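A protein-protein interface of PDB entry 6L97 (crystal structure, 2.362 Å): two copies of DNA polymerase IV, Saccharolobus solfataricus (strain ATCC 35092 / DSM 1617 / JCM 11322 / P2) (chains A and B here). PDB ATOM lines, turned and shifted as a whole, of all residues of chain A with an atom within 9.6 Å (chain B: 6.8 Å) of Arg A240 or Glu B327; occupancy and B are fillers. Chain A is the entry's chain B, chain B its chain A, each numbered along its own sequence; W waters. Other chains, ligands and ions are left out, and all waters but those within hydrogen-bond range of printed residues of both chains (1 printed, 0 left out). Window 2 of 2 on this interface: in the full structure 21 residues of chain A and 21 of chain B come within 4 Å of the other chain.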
ATOM      1  N   GLN A  82     -13.642  -3.893  -0.769  1.00  0.00           N
ATOM      2  CA  GLN A  82     -12.813  -3.207   0.218  1.00  0.00           C
ATOM      3  C   GLN A  82     -12.426  -1.810  -0.249  1.00  0.00           C
ATOM      4  O   GLN A  82     -12.431  -0.861   0.543  1.00  0.00           O
ATOM      5  CB  GLN A  82     -11.560  -4.030   0.516  1.00  0.00           C
ATOM      6  CG  GLN A  82     -10.667  -3.404   1.573  1.00  0.00           C
ATOM      7  CD  GLN A  82     -11.419  -3.120   2.865  1.00  0.00           C
ATOM      8  OE1 GLN A  82     -11.563  -1.967   3.277  1.00  0.00           O
ATOM      9  NE2 GLN A  82     -11.904  -4.177   3.508  1.00  0.00           N
ATOM     10  N   ARG A  93     -15.058  10.699   7.046  1.00  0.00           N
ATOM     11  CA  ARG A  93     -14.195  11.419   7.980  1.00  0.00           C
ATOM     12  C   ARG A  93     -14.198  12.918   7.708  1.00  0.00           C
ATOM     13  O   ARG A  93     -13.945  13.713   8.622  1.00  0.00           O
ATOM     14  CB  ARG A  93     -12.766  10.871   7.918  1.00  0.00           C
ATOM     15  CG  ARG A  93     -12.678   9.362   8.070  1.00  0.00           C
ATOM     16  CD  ARG A  93     -11.251   8.847   7.904  1.00  0.00           C
ATOM     17  NE  ARG A  93     -10.677   8.462   9.189  1.00  0.00           N
ATOM     18  CZ  ARG A  93     -10.414   7.208   9.545  1.00  0.00           C
ATOM     19  NH1 ARG A  93     -10.665   6.211   8.704  1.00  0.00           N
ATOM     20  NH2 ARG A  93      -9.899   6.951  10.743  1.00  0.00           N
ATOM     21  N   GLU A  97     -14.855  14.022  12.573  1.00  0.00           N
ATOM     22  CA  GLU A  97     -13.572  13.752  13.118  1.00  0.00           C
ATOM     23  C   GLU A  97     -13.509  12.427  13.857  1.00  0.00           C
ATOM     24  O   GLU A  97     -12.521  11.723  13.796  1.00  0.00           O
ATOM     25  CB  GLU A  97     -13.198  14.946  14.010  1.00  0.00           C
ATOM     26  CG  GLU A  97     -13.944  15.151  15.328  1.00  0.00           C
ATOM     27  CD  GLU A  97     -15.463  15.367  15.229  1.00  0.00           C
ATOM     28  OE1 GLU A  97     -16.122  14.678  14.443  1.00  0.00           O
ATOM     29  OE2 GLU A  97     -16.030  16.179  15.998  1.00  0.00           O
ATOM     30  N   LYS A  98     -14.600  12.084  14.518  1.00  0.00           N
ATOM     31  CA  LYS A  98     -14.700  10.856  15.264  1.00  0.00           C
ATOM     32  C   LYS A  98     -15.511   9.837  14.539  1.00  0.00           C
ATOM     33  O   LYS A  98     -16.643  10.039  14.318  1.00  0.00           O
ATOM     34  CB  LYS A  98     -15.391  11.119  16.566  1.00  0.00           C
ATOM     35  CG  LYS A  98     -15.223  12.512  17.044  1.00  0.00           C
ATOM     36  CD  LYS A  98     -15.269  12.570  18.529  1.00  0.00           C
ATOM     37  CE  LYS A  98     -14.197  13.495  19.042  1.00  0.00           C
ATOM     38  NZ  LYS A  98     -14.771  14.634  19.801  1.00  0.00           N
ATOM     39  N   ILE A  99     -14.934   8.713  14.214  1.00  0.00           N
ATOM     40  CA  ILE A  99     -15.643   7.717  13.509  1.00  0.00           C
ATOM     41  C   ILE A  99     -15.098   6.376  13.843  1.00  0.00           C
ATOM     42  O   ILE A  99     -13.963   6.245  14.061  1.00  0.00           O
ATOM     43  CB  ILE A  99     -15.480   7.942  12.027  1.00  0.00           C
ATOM     44  CG1 ILE A  99     -16.081   6.808  11.268  1.00  0.00           C
ATOM     45  CG2 ILE A  99     -14.030   8.002  11.678  1.00  0.00           C
ATOM     46  CD1 ILE A  99     -15.974   6.989   9.791  1.00  0.00           C
ATOM     47  N   GLU A 100     -15.937   5.376  13.853  1.00  0.00           N
ATOM     48  CA  GLU A 100     -15.564   4.011  14.191  1.00  0.00           C
ATOM     49  C   GLU A 100     -16.036   3.111  13.059  1.00  0.00           C
ATOM     50  O   GLU A 100     -17.244   2.956  12.845  1.00  0.00           O
ATOM     51  CB  GLU A 100     -16.173   3.594  15.529  1.00  0.00           C
ATOM     52  CG  GLU A 100     -16.044   2.114  15.844  1.00  0.00           C
ATOM     53  CD  GLU A 100     -16.668   1.745  17.182  1.00  0.00           C
ATOM     54  OE1 GLU A 100     -16.968   0.550  17.393  1.00  0.00           O
ATOM     55  OE2 GLU A 100     -16.850   2.648  18.026  1.00  0.00           O
ATOM     56  N   ILE A 101     -15.087   2.534  12.323  1.00  0.00           N
ATOM     57  CA  ILE A 101     -15.411   1.604  11.245  1.00  0.00           C
ATOM     58  C   ILE A 101     -15.674   0.250  11.896  1.00  0.00           C
ATOM     59  O   ILE A 101     -14.743  -0.478  12.241  1.00  0.00           O
ATOM     60  CB  ILE A 101     -14.302   1.530  10.195  1.00  0.00           C
ATOM     61  CG1 ILE A 101     -14.131   2.885   9.510  1.00  0.00           C
ATOM     62  CG2 ILE A 101     -14.608   0.456   9.160  1.00  0.00           C
ATOM     63  CD1 ILE A 101     -12.973   3.701  10.047  1.00  0.00           C
ATOM     64  N   ALA A 102     -16.952  -0.080  12.083  1.00  0.00           N
ATOM     65  CA  ALA A 102     -17.318  -1.323  12.751  1.00  0.00           C
ATOM     66  C   ALA A 102     -17.119  -2.541  11.861  1.00  0.00           C
ATOM     67  O   ALA A 102     -16.820  -3.627  12.368  1.00  0.00           O
ATOM     68  CB  ALA A 102     -18.773  -1.258  13.225  1.00  0.00           C
ATOM     69  N   SER A 103     -17.280  -2.391  10.551  1.00  0.00           N
ATOM     70  CA  SER A 103     -17.116  -3.510   9.628  1.00  0.00           C
ATOM     71  C   SER A 103     -17.017  -2.951   8.214  1.00  0.00           C
ATOM     72  O   SER A 103     -16.878  -1.738   8.013  1.00  0.00           O
ATOM     73  CB  SER A 103     -18.265  -4.509   9.749  1.00  0.00           C
ATOM     74  OG  SER A 103     -19.478  -3.911   9.337  1.00  0.00           O
ATOM     75  N   TYR A 108     -19.872   4.271  12.543  1.00  0.00           N
ATOM     76  CA  TYR A 108     -20.514   5.180  13.483  1.00  0.00           C
ATOM     77  C   TYR A 108     -19.791   6.518  13.487  1.00  0.00           C
ATOM     78  O   TYR A 108     -18.560   6.566  13.442  1.00  0.00           O
ATOM     79  CB  TYR A 108     -20.507   4.610  14.901  1.00  0.00           C
ATOM     80  CG  TYR A 108     -21.314   3.352  15.079  1.00  0.00           C
ATOM     81  CD1 TYR A 108     -20.772   2.109  14.774  1.00  0.00           C
ATOM     82  CD2 TYR A 108     -22.616   3.401  15.569  1.00  0.00           C
ATOM     83  CE1 TYR A 108     -21.501   0.951  14.942  1.00  0.00           C
ATOM     84  CE2 TYR A 108     -23.357   2.247  15.740  1.00  0.00           C
ATOM     85  CZ  TYR A 108     -22.792   1.026  15.426  1.00  0.00           C
ATOM     86  OH  TYR A 108     -23.524  -0.125  15.593  1.00  0.00           O
ATOM     87  N   ILE A 237     -17.717   6.549  20.919  1.00  0.00           N
ATOM     88  CA  ILE A 237     -17.239   6.117  19.611  1.00  0.00           C
ATOM     89  C   ILE A 237     -15.724   5.966  19.681  1.00  0.00           C
ATOM     90  O   ILE A 237     -15.004   6.934  19.942  1.00  0.00           O
ATOM     91  CB  ILE A 237     -17.656   7.109  18.517  1.00  0.00           C
ATOM     92  CG1 ILE A 237     -19.113   7.537  18.714  1.00  0.00           C
ATOM     93  CG2 ILE A 237     -17.489   6.488  17.142  1.00  0.00           C
ATOM     94  CD1 ILE A 237     -20.122   6.424  18.491  1.00  0.00           C
ATOM     95  N   ARG A 238     -15.242   4.745  19.459  1.00  0.00           N
ATOM     96  CA  ARG A 238     -13.822   4.426  19.572  1.00  0.00           C
ATOM     97  C   ARG A 238     -13.148   4.758  18.246  1.00  0.00           C
ATOM     98  O   ARG A 238     -13.194   3.975  17.294  1.00  0.00           O
ATOM     99  CB  ARG A 238     -13.628   2.962  19.949  1.00  0.00           C
ATOM    100  CG  ARG A 238     -14.131   2.612  21.347  1.00  0.00           C
ATOM    101  CD  ARG A 238     -13.016   2.063  22.227  1.00  0.00           C
ATOM    102  NE  ARG A 238     -13.192   2.428  23.631  1.00  0.00           N
ATOM    103  CZ  ARG A 238     -13.478   1.567  24.604  1.00  0.00           C
ATOM    104  NH1 ARG A 238     -13.616   1.996  25.852  1.00  0.00           N
ATOM    105  NH2 ARG A 238     -13.621   0.277  24.332  1.00  0.00           N
ATOM    106  N   THR A 239     -12.528   5.934  18.187  1.00  0.00           N
ATOM    107  CA  THR A 239     -11.813   6.387  17.005  1.00  0.00           C
ATOM    108  C   THR A 239     -10.370   5.902  17.073  1.00  0.00           C
ATOM    109  O   THR A 239      -9.699   6.076  18.095  1.00  0.00           O
ATOM    110  CB  THR A 239     -11.859   7.913  16.901  1.00  0.00           C
ATOM    111  OG1 THR A 239     -13.125   8.388  17.376  1.00  0.00           O
ATOM    112  CG2 THR A 239     -11.663   8.363  15.462  1.00  0.00           C
ATOM    113  N   ARG A 240      -9.902   5.289  15.989  1.00  0.00           N
ATOM    114  CA  ARG A 240      -8.546   4.760  15.925  1.00  0.00           C
ATOM    115  C   ARG A 240      -7.607   5.798  15.322  1.00  0.00           C
ATOM    116  O   ARG A 240      -7.858   6.313  14.228  1.00  0.00           O
ATOM    117  CB  ARG A 240      -8.507   3.470  15.104  1.00  0.00           C
ATOM    118  CG  ARG A 240      -8.605   2.207  15.945  1.00  0.00           C
ATOM    119  CD  ARG A 240      -9.108   1.024  15.135  1.00  0.00           C
ATOM    120  NE  ARG A 240      -9.327  -0.145  15.984  1.00  0.00           N
ATOM    121  CZ  ARG A 240      -9.848  -1.290  15.562  1.00  0.00           C
ATOM    122  NH1 ARG A 240     -10.207  -1.429  14.293  1.00  0.00           N
ATOM    123  NH2 ARG A 240     -10.000  -2.301  16.405  1.00  0.00           N
ATOM    124  N   VAL A 241      -6.530   6.099  16.041  1.00  0.00           N
ATOM    125  CA  VAL A 241      -5.499   7.027  15.592  1.00  0.00           C
ATOM    126  C   VAL A 241      -4.143   6.360  15.787  1.00  0.00           C
ATOM    127  O   VAL A 241      -3.909   5.694  16.801  1.00  0.00           O
ATOM    128  CB  VAL A 241      -5.574   8.370  16.352  1.00  0.00           C
ATOM    129  CG1 VAL A 241      -5.550   8.138  17.856  1.00  0.00           C
ATOM    130  CG2 VAL A 241      -4.445   9.297  15.924  1.00  0.00           C
ATOM    131  N   ARG A 242      -3.256   6.521  14.810  1.00  0.00           N
ATOM    132  CA  ARG A 242      -1.977   5.820  14.825  1.00  0.00           C
ATOM    133  C   ARG A 242      -0.996   6.571  15.723  1.00  0.00           C
ATOM    134  O   ARG A 242      -0.548   7.673  15.386  1.00  0.00           O
ATOM    135  CB  ARG A 242      -1.440   5.671  13.405  1.00  0.00           C
ATOM    136  CG  ARG A 242      -0.469   4.516  13.247  1.00  0.00           C
ATOM    137  CD  ARG A 242      -0.495   3.952  11.839  1.00  0.00           C
ATOM    138  NE  ARG A 242      -1.686   3.149  11.578  1.00  0.00           N
ATOM    139  CZ  ARG A 242      -1.951   2.578  10.407  1.00  0.00           C
ATOM    140  NH1 ARG A 242      -1.111   2.726   9.389  1.00  0.00           N
ATOM    141  NH2 ARG A 242      -3.053   1.859  10.252  1.00  0.00           N
ATOM    142  N   LYS A 243      -0.665   5.968  16.870  1.00  0.00           N
ATOM    143  CA  LYS A 243       0.267   6.590  17.810  1.00  0.00           C
ATOM    144  C   LYS A 243       1.638   6.816  17.180  1.00  0.00           C
ATOM    145  O   LYS A 243       2.242   7.882  17.348  1.00  0.00           O
ATOM    146  CB  LYS A 243       0.400   5.724  19.065  1.00  0.00           C
ATOM    147  CG  LYS A 243       1.070   4.368  18.812  1.00  0.00           C
ATOM    148  CD  LYS A 243       1.970   3.952  19.961  1.00  0.00           C
ATOM    149  CE  LYS A 243       2.812   2.741  19.590  1.00  0.00           C
ATOM    150  NZ  LYS A 243       4.122   2.744  20.304  1.00  0.00           N
ATOM    151  N   LYS A 275       4.992   7.186   4.792  1.00  0.00           N
ATOM    152  CA  LYS A 275       3.732   6.867   5.450  1.00  0.00           C
ATOM    153  C   LYS A 275       3.281   7.954   6.417  1.00  0.00           C
ATOM    154  O   LYS A 275       2.160   7.873   6.936  1.00  0.00           O
ATOM    155  CB  LYS A 275       3.852   5.531   6.198  1.00  0.00           C
ATOM    156  CG  LYS A 275       4.268   4.365   5.315  1.00  0.00           C
ATOM    157  CD  LYS A 275       3.707   3.046   5.816  1.00  0.00           C
ATOM    158  CE  LYS A 275       4.469   2.530   7.024  1.00  0.00           C
ATOM    159  NZ  LYS A 275       3.787   1.340   7.622  1.00  0.00           N
ATOM    160  N   ARG A 279       2.726  14.821   8.180  1.00  0.00           N
ATOM    161  CA  ARG A 279       2.956  14.729   9.612  1.00  0.00           C
ATOM    162  C   ARG A 279       4.449  14.834   9.875  1.00  0.00           C
ATOM    163  O   ARG A 279       5.273  14.430   9.049  1.00  0.00           O
ATOM    164  CB  ARG A 279       2.421  13.425  10.206  1.00  0.00           C
ATOM    165  CG  ARG A 279       0.947  13.463  10.546  1.00  0.00           C
ATOM    166  CD  ARG A 279       0.318  12.086  10.408  1.00  0.00           C
ATOM    167  NE  ARG A 279      -0.389  11.687  11.622  1.00  0.00           N
ATOM    168  CZ  ARG A 279      -1.029  10.532  11.767  1.00  0.00           C
ATOM    169  NH1 ARG A 279      -1.053   9.658  10.766  1.00  0.00           N
ATOM    170  NH2 ARG A 279      -1.647  10.254  12.912  1.00  0.00           N
ATOM    171  N   ARG B 256      -5.429 -11.955  14.206  1.00  0.00           N
ATOM    172  CA  ARG B 256      -6.045 -11.023  15.140  1.00  0.00           C
ATOM    173  C   ARG B 256      -6.871 -11.751  16.190  1.00  0.00           C
ATOM    174  O   ARG B 256      -7.644 -11.108  16.909  1.00  0.00           O
ATOM    175  CB  ARG B 256      -6.920 -10.002  14.403  1.00  0.00           C
ATOM    176  CG  ARG B 256      -6.153  -8.804  13.871  1.00  0.00           C
ATOM    177  CD  ARG B 256      -7.068  -7.818  13.156  1.00  0.00           C
ATOM    178  NE  ARG B 256      -7.937  -7.105  14.090  1.00  0.00           N
ATOM    179  CZ  ARG B 256      -7.572  -6.025  14.774  1.00  0.00           C
ATOM    180  NH1 ARG B 256      -8.427  -5.437  15.598  1.00  0.00           N
ATOM    181  NH2 ARG B 256      -6.347  -5.530  14.637  1.00  0.00           N
ATOM    182  N   ILE B 322      -4.023  -3.627  22.413  1.00  0.00           N
ATOM    183  CA  ILE B 322      -3.445  -3.417  21.093  1.00  0.00           C
ATOM    184  C   ILE B 322      -4.468  -3.716  20.008  1.00  0.00           C
ATOM    185  O   ILE B 322      -4.598  -2.968  19.032  1.00  0.00           O
ATOM    186  CB  ILE B 322      -2.182  -4.277  20.930  1.00  0.00           C
ATOM    187  CG1 ILE B 322      -1.046  -3.696  21.773  1.00  0.00           C
ATOM    188  CG2 ILE B 322      -1.802  -4.397  19.455  1.00  0.00           C
ATOM    189  CD1 ILE B 322       0.160  -4.578  21.834  1.00  0.00           C
ATOM    190  N   LEU B 323      -5.215  -4.813  20.159  1.00  0.00           N
ATOM    191  CA  LEU B 323      -6.179  -5.186  19.131  1.00  0.00           C
ATOM    192  C   LEU B 323      -7.334  -4.191  19.038  1.00  0.00           C
ATOM    193  O   LEU B 323      -7.853  -3.959  17.940  1.00  0.00           O
ATOM    194  CB  LEU B 323      -6.695  -6.599  19.395  1.00  0.00           C
ATOM    195  CG  LEU B 323      -5.617  -7.680  19.276  1.00  0.00           C
ATOM    196  CD1 LEU B 323      -6.033  -8.944  20.003  1.00  0.00           C
ATOM    197  CD2 LEU B 323      -5.312  -7.975  17.819  1.00  0.00           C
ATOM    198  N   GLU B 324      -7.739  -3.583  20.160  1.00  0.00           N
ATOM    199  CA  GLU B 324      -8.831  -2.610  20.114  1.00  0.00           C
ATOM    200  C   GLU B 324      -8.424  -1.328  19.398  1.00  0.00           C
ATOM    201  O   GLU B 324      -9.255  -0.713  18.719  1.00  0.00           O
ATOM    202  CB  GLU B 324      -9.317  -2.275  21.532  1.00  0.00           C
ATOM    203  CG  GLU B 324      -9.420  -3.469  22.470  1.00  0.00           C
ATOM    204  CD  GLU B 324      -9.920  -3.102  23.866  1.00  0.00           C
ATOM    205  OE1 GLU B 324      -9.537  -2.028  24.381  1.00  0.00           O
ATOM    206  OE2 GLU B 324     -10.676  -3.902  24.459  1.00  0.00           O
ATOM    207  N   GLU B 325      -7.166  -0.910  19.531  1.00  0.00           N
ATOM    208  CA  GLU B 325      -6.723   0.392  19.051  1.00  0.00           C
ATOM    209  C   GLU B 325      -5.998   0.338  17.710  1.00  0.00           C
ATOM    210  O   GLU B 325      -5.576   1.386  17.214  1.00  0.00           O
ATOM    211  CB  GLU B 325      -5.821   1.053  20.097  1.00  0.00           C
ATOM    212  CG  GLU B 325      -6.483   1.225  21.455  1.00  0.00           C
ATOM    213  CD  GLU B 325      -5.716   2.155  22.382  1.00  0.00           C
ATOM    214  OE1 GLU B 325      -4.633   2.644  21.990  1.00  0.00           O
ATOM    215  OE2 GLU B 325      -6.205   2.401  23.505  1.00  0.00           O
ATOM    216  N   ASP B 326      -5.837  -0.846  17.116  1.00  0.00           N
ATOM    217  CA  ASP B 326      -5.170  -0.986  15.827  1.00  0.00           C
ATOM    218  C   ASP B 326      -5.896  -2.035  15.000  1.00  0.00           C
ATOM    219  O   ASP B 326      -6.207  -3.123  15.494  1.00  0.00           O
ATOM    220  CB  ASP B 326      -3.690  -1.378  15.988  1.00  0.00           C
ATOM    221  CG  ASP B 326      -2.815  -0.873  14.836  1.00  0.00           C
ATOM    222  OD1 ASP B 326      -3.046  -1.267  13.671  1.00  0.00           O
ATOM    223  OD2 ASP B 326      -1.889  -0.078  15.099  1.00  0.00           O
ATOM    224  N   GLU B 327      -6.160  -1.704  13.737  1.00  0.00           N
ATOM    225  CA  GLU B 327      -6.907  -2.588  12.849  1.00  0.00           C
ATOM    226  C   GLU B 327      -6.029  -3.578  12.089  1.00  0.00           C
ATOM    227  O   GLU B 327      -6.559  -4.543  11.527  1.00  0.00           O
ATOM    228  CB  GLU B 327      -7.716  -1.760  11.843  1.00  0.00           C
ATOM    229  CG  GLU B 327      -6.943  -1.367  10.589  1.00  0.00           C
ATOM    230  CD  GLU B 327      -5.972  -0.222  10.827  1.00  0.00           C
ATOM    231  OE1 GLU B 327      -5.091   0.004   9.967  1.00  0.00           O
ATOM    232  OE2 GLU B 327      -6.090   0.450  11.872  1.00  0.00           O
ATOM    233  N   ARG B 328      -4.713  -3.369  12.052  1.00  0.00           N
ATOM    234  CA  ARG B 328      -3.849  -4.240  11.267  1.00  0.00           C
ATOM    235  C   ARG B 328      -3.725  -5.614  11.919  1.00  0.00           C
ATOM    236  O   ARG B 328      -3.945  -5.788  13.121  1.00  0.00           O
ATOM    237  CB  ARG B 328      -2.461  -3.618  11.104  1.00  0.00           C
ATOM    238  CG  ARG B 328      -2.424  -2.377  10.228  1.00  0.00           C
ATOM    239  CD  ARG B 328      -1.104  -1.641  10.369  1.00  0.00           C
ATOM    240  NE  ARG B 328      -0.945  -1.086  11.709  1.00  0.00           N
ATOM    241  CZ  ARG B 328      -0.012  -0.205  12.048  1.00  0.00           C
ATOM    242  NH1 ARG B 328       0.854   0.234  11.142  1.00  0.00           N
ATOM    243  NH2 ARG B 328       0.053   0.245  13.291  1.00  0.00           N
ATOM    244  N   LYS B 329      -3.370  -6.600  11.102  1.00  0.00           N
ATOM    245  CA  LYS B 329      -3.080  -7.930  11.614  1.00  0.00           C
ATOM    246  C   LYS B 329      -1.670  -7.968  12.188  1.00  0.00           C
ATOM    247  O   LYS B 329      -0.782  -7.230  11.756  1.00  0.00           O
ATOM    248  CB  LYS B 329      -3.227  -8.983  10.515  1.00  0.00           C
ATOM    249  CG  LYS B 329      -4.494  -8.853   9.681  1.00  0.00           C
ATOM    250  CD  LYS B 329      -4.562  -9.929   8.606  1.00  0.00           C
ATOM    251  CE  LYS B 329      -4.762 -11.314   9.209  1.00  0.00           C
ATOM    252  NZ  LYS B 329      -4.929 -12.370   8.164  1.00  0.00           N
HETATM  253  O   HOH W   1      -3.982   1.712  12.474  1.00  0.00           O
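Arg A240 touches six residues of chain B. Of the printed residues of chain A, Glu B325 touches Arg A240. Of the printed residues of chain A, Arg B328 touches Arg A242. Printed residues of chain A within 4 Å of Glu B324: Arg A240. The nearest residue of chain B that does not touch Arg A240 is Ile B322 (6.0 Å). The nearest printed residue of chain A that does not touch Arg B256 is Ile A101 (8.7 Å).
Of the 19 printed residues of chain A, 2 touch a printed residue of chain B. Of the 9 printed residues of chain B, 7 touch a printed residue of chain A. Along chain B the printed residues that touch a printed residue of chain A span positions 256 to 328.
The backbone carbonyl oxygen (O) of Arg B328 lies within hydrogen-bond range of the guanidinium group (NH2) of Arg B256 (2.9 Å). NH2 of Arg B256 sits close to O of Glu B327, at 3.3 Å. The backbone carbonyl oxygen of Leu B323 is in hydrogen-bond range of the guanidinium group of Arg B256 (2.8 Å). NH2 of Arg B256 lies within hydrogen-bond range of O of Asp B326 (2.6 Å). The side-chain carboxylate (OD2) of Asp B326 lies within salt-bridge range of the guanidinium group (NH2) of Arg B328 (2.7 Å).
O of Glu B324 lies within hydrogen-bond range of NE of Arg A240 (2.8 Å). OE1 of Glu B327 is in salt-bridge range of NH2 of Arg A242 (2.8 Å). The guanidinium group (NH2) of Arg A240 sits at hydrogen-bond distance from the backbone carbonyl oxygen (O) of Leu B323, 3.1 Å away.
Water W1 lies within hydrogen-bond range of the guanidinium group of Arg A242 (2.4 Å), the side-chain carboxylate of Glu B327 (2.5 Å) and the side-chain carboxylate of Asp B326 (3.3 Å).
Arg A240 touches Arg B256. Glu B325 touches Arg A240 (O to CG, 3.4 Å). Arg A240 touches Asp B326. NH1 of Arg A240 touches CB of Glu B327, 3.5 Å away. NH1 of Arg B328 touches NH1 of Arg A242, at 3.6 Å.
No position is printed for both chains. Of the 8 pairs that touch across the chains among the printed residues, none has its exchanged pair printed and touching as well.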
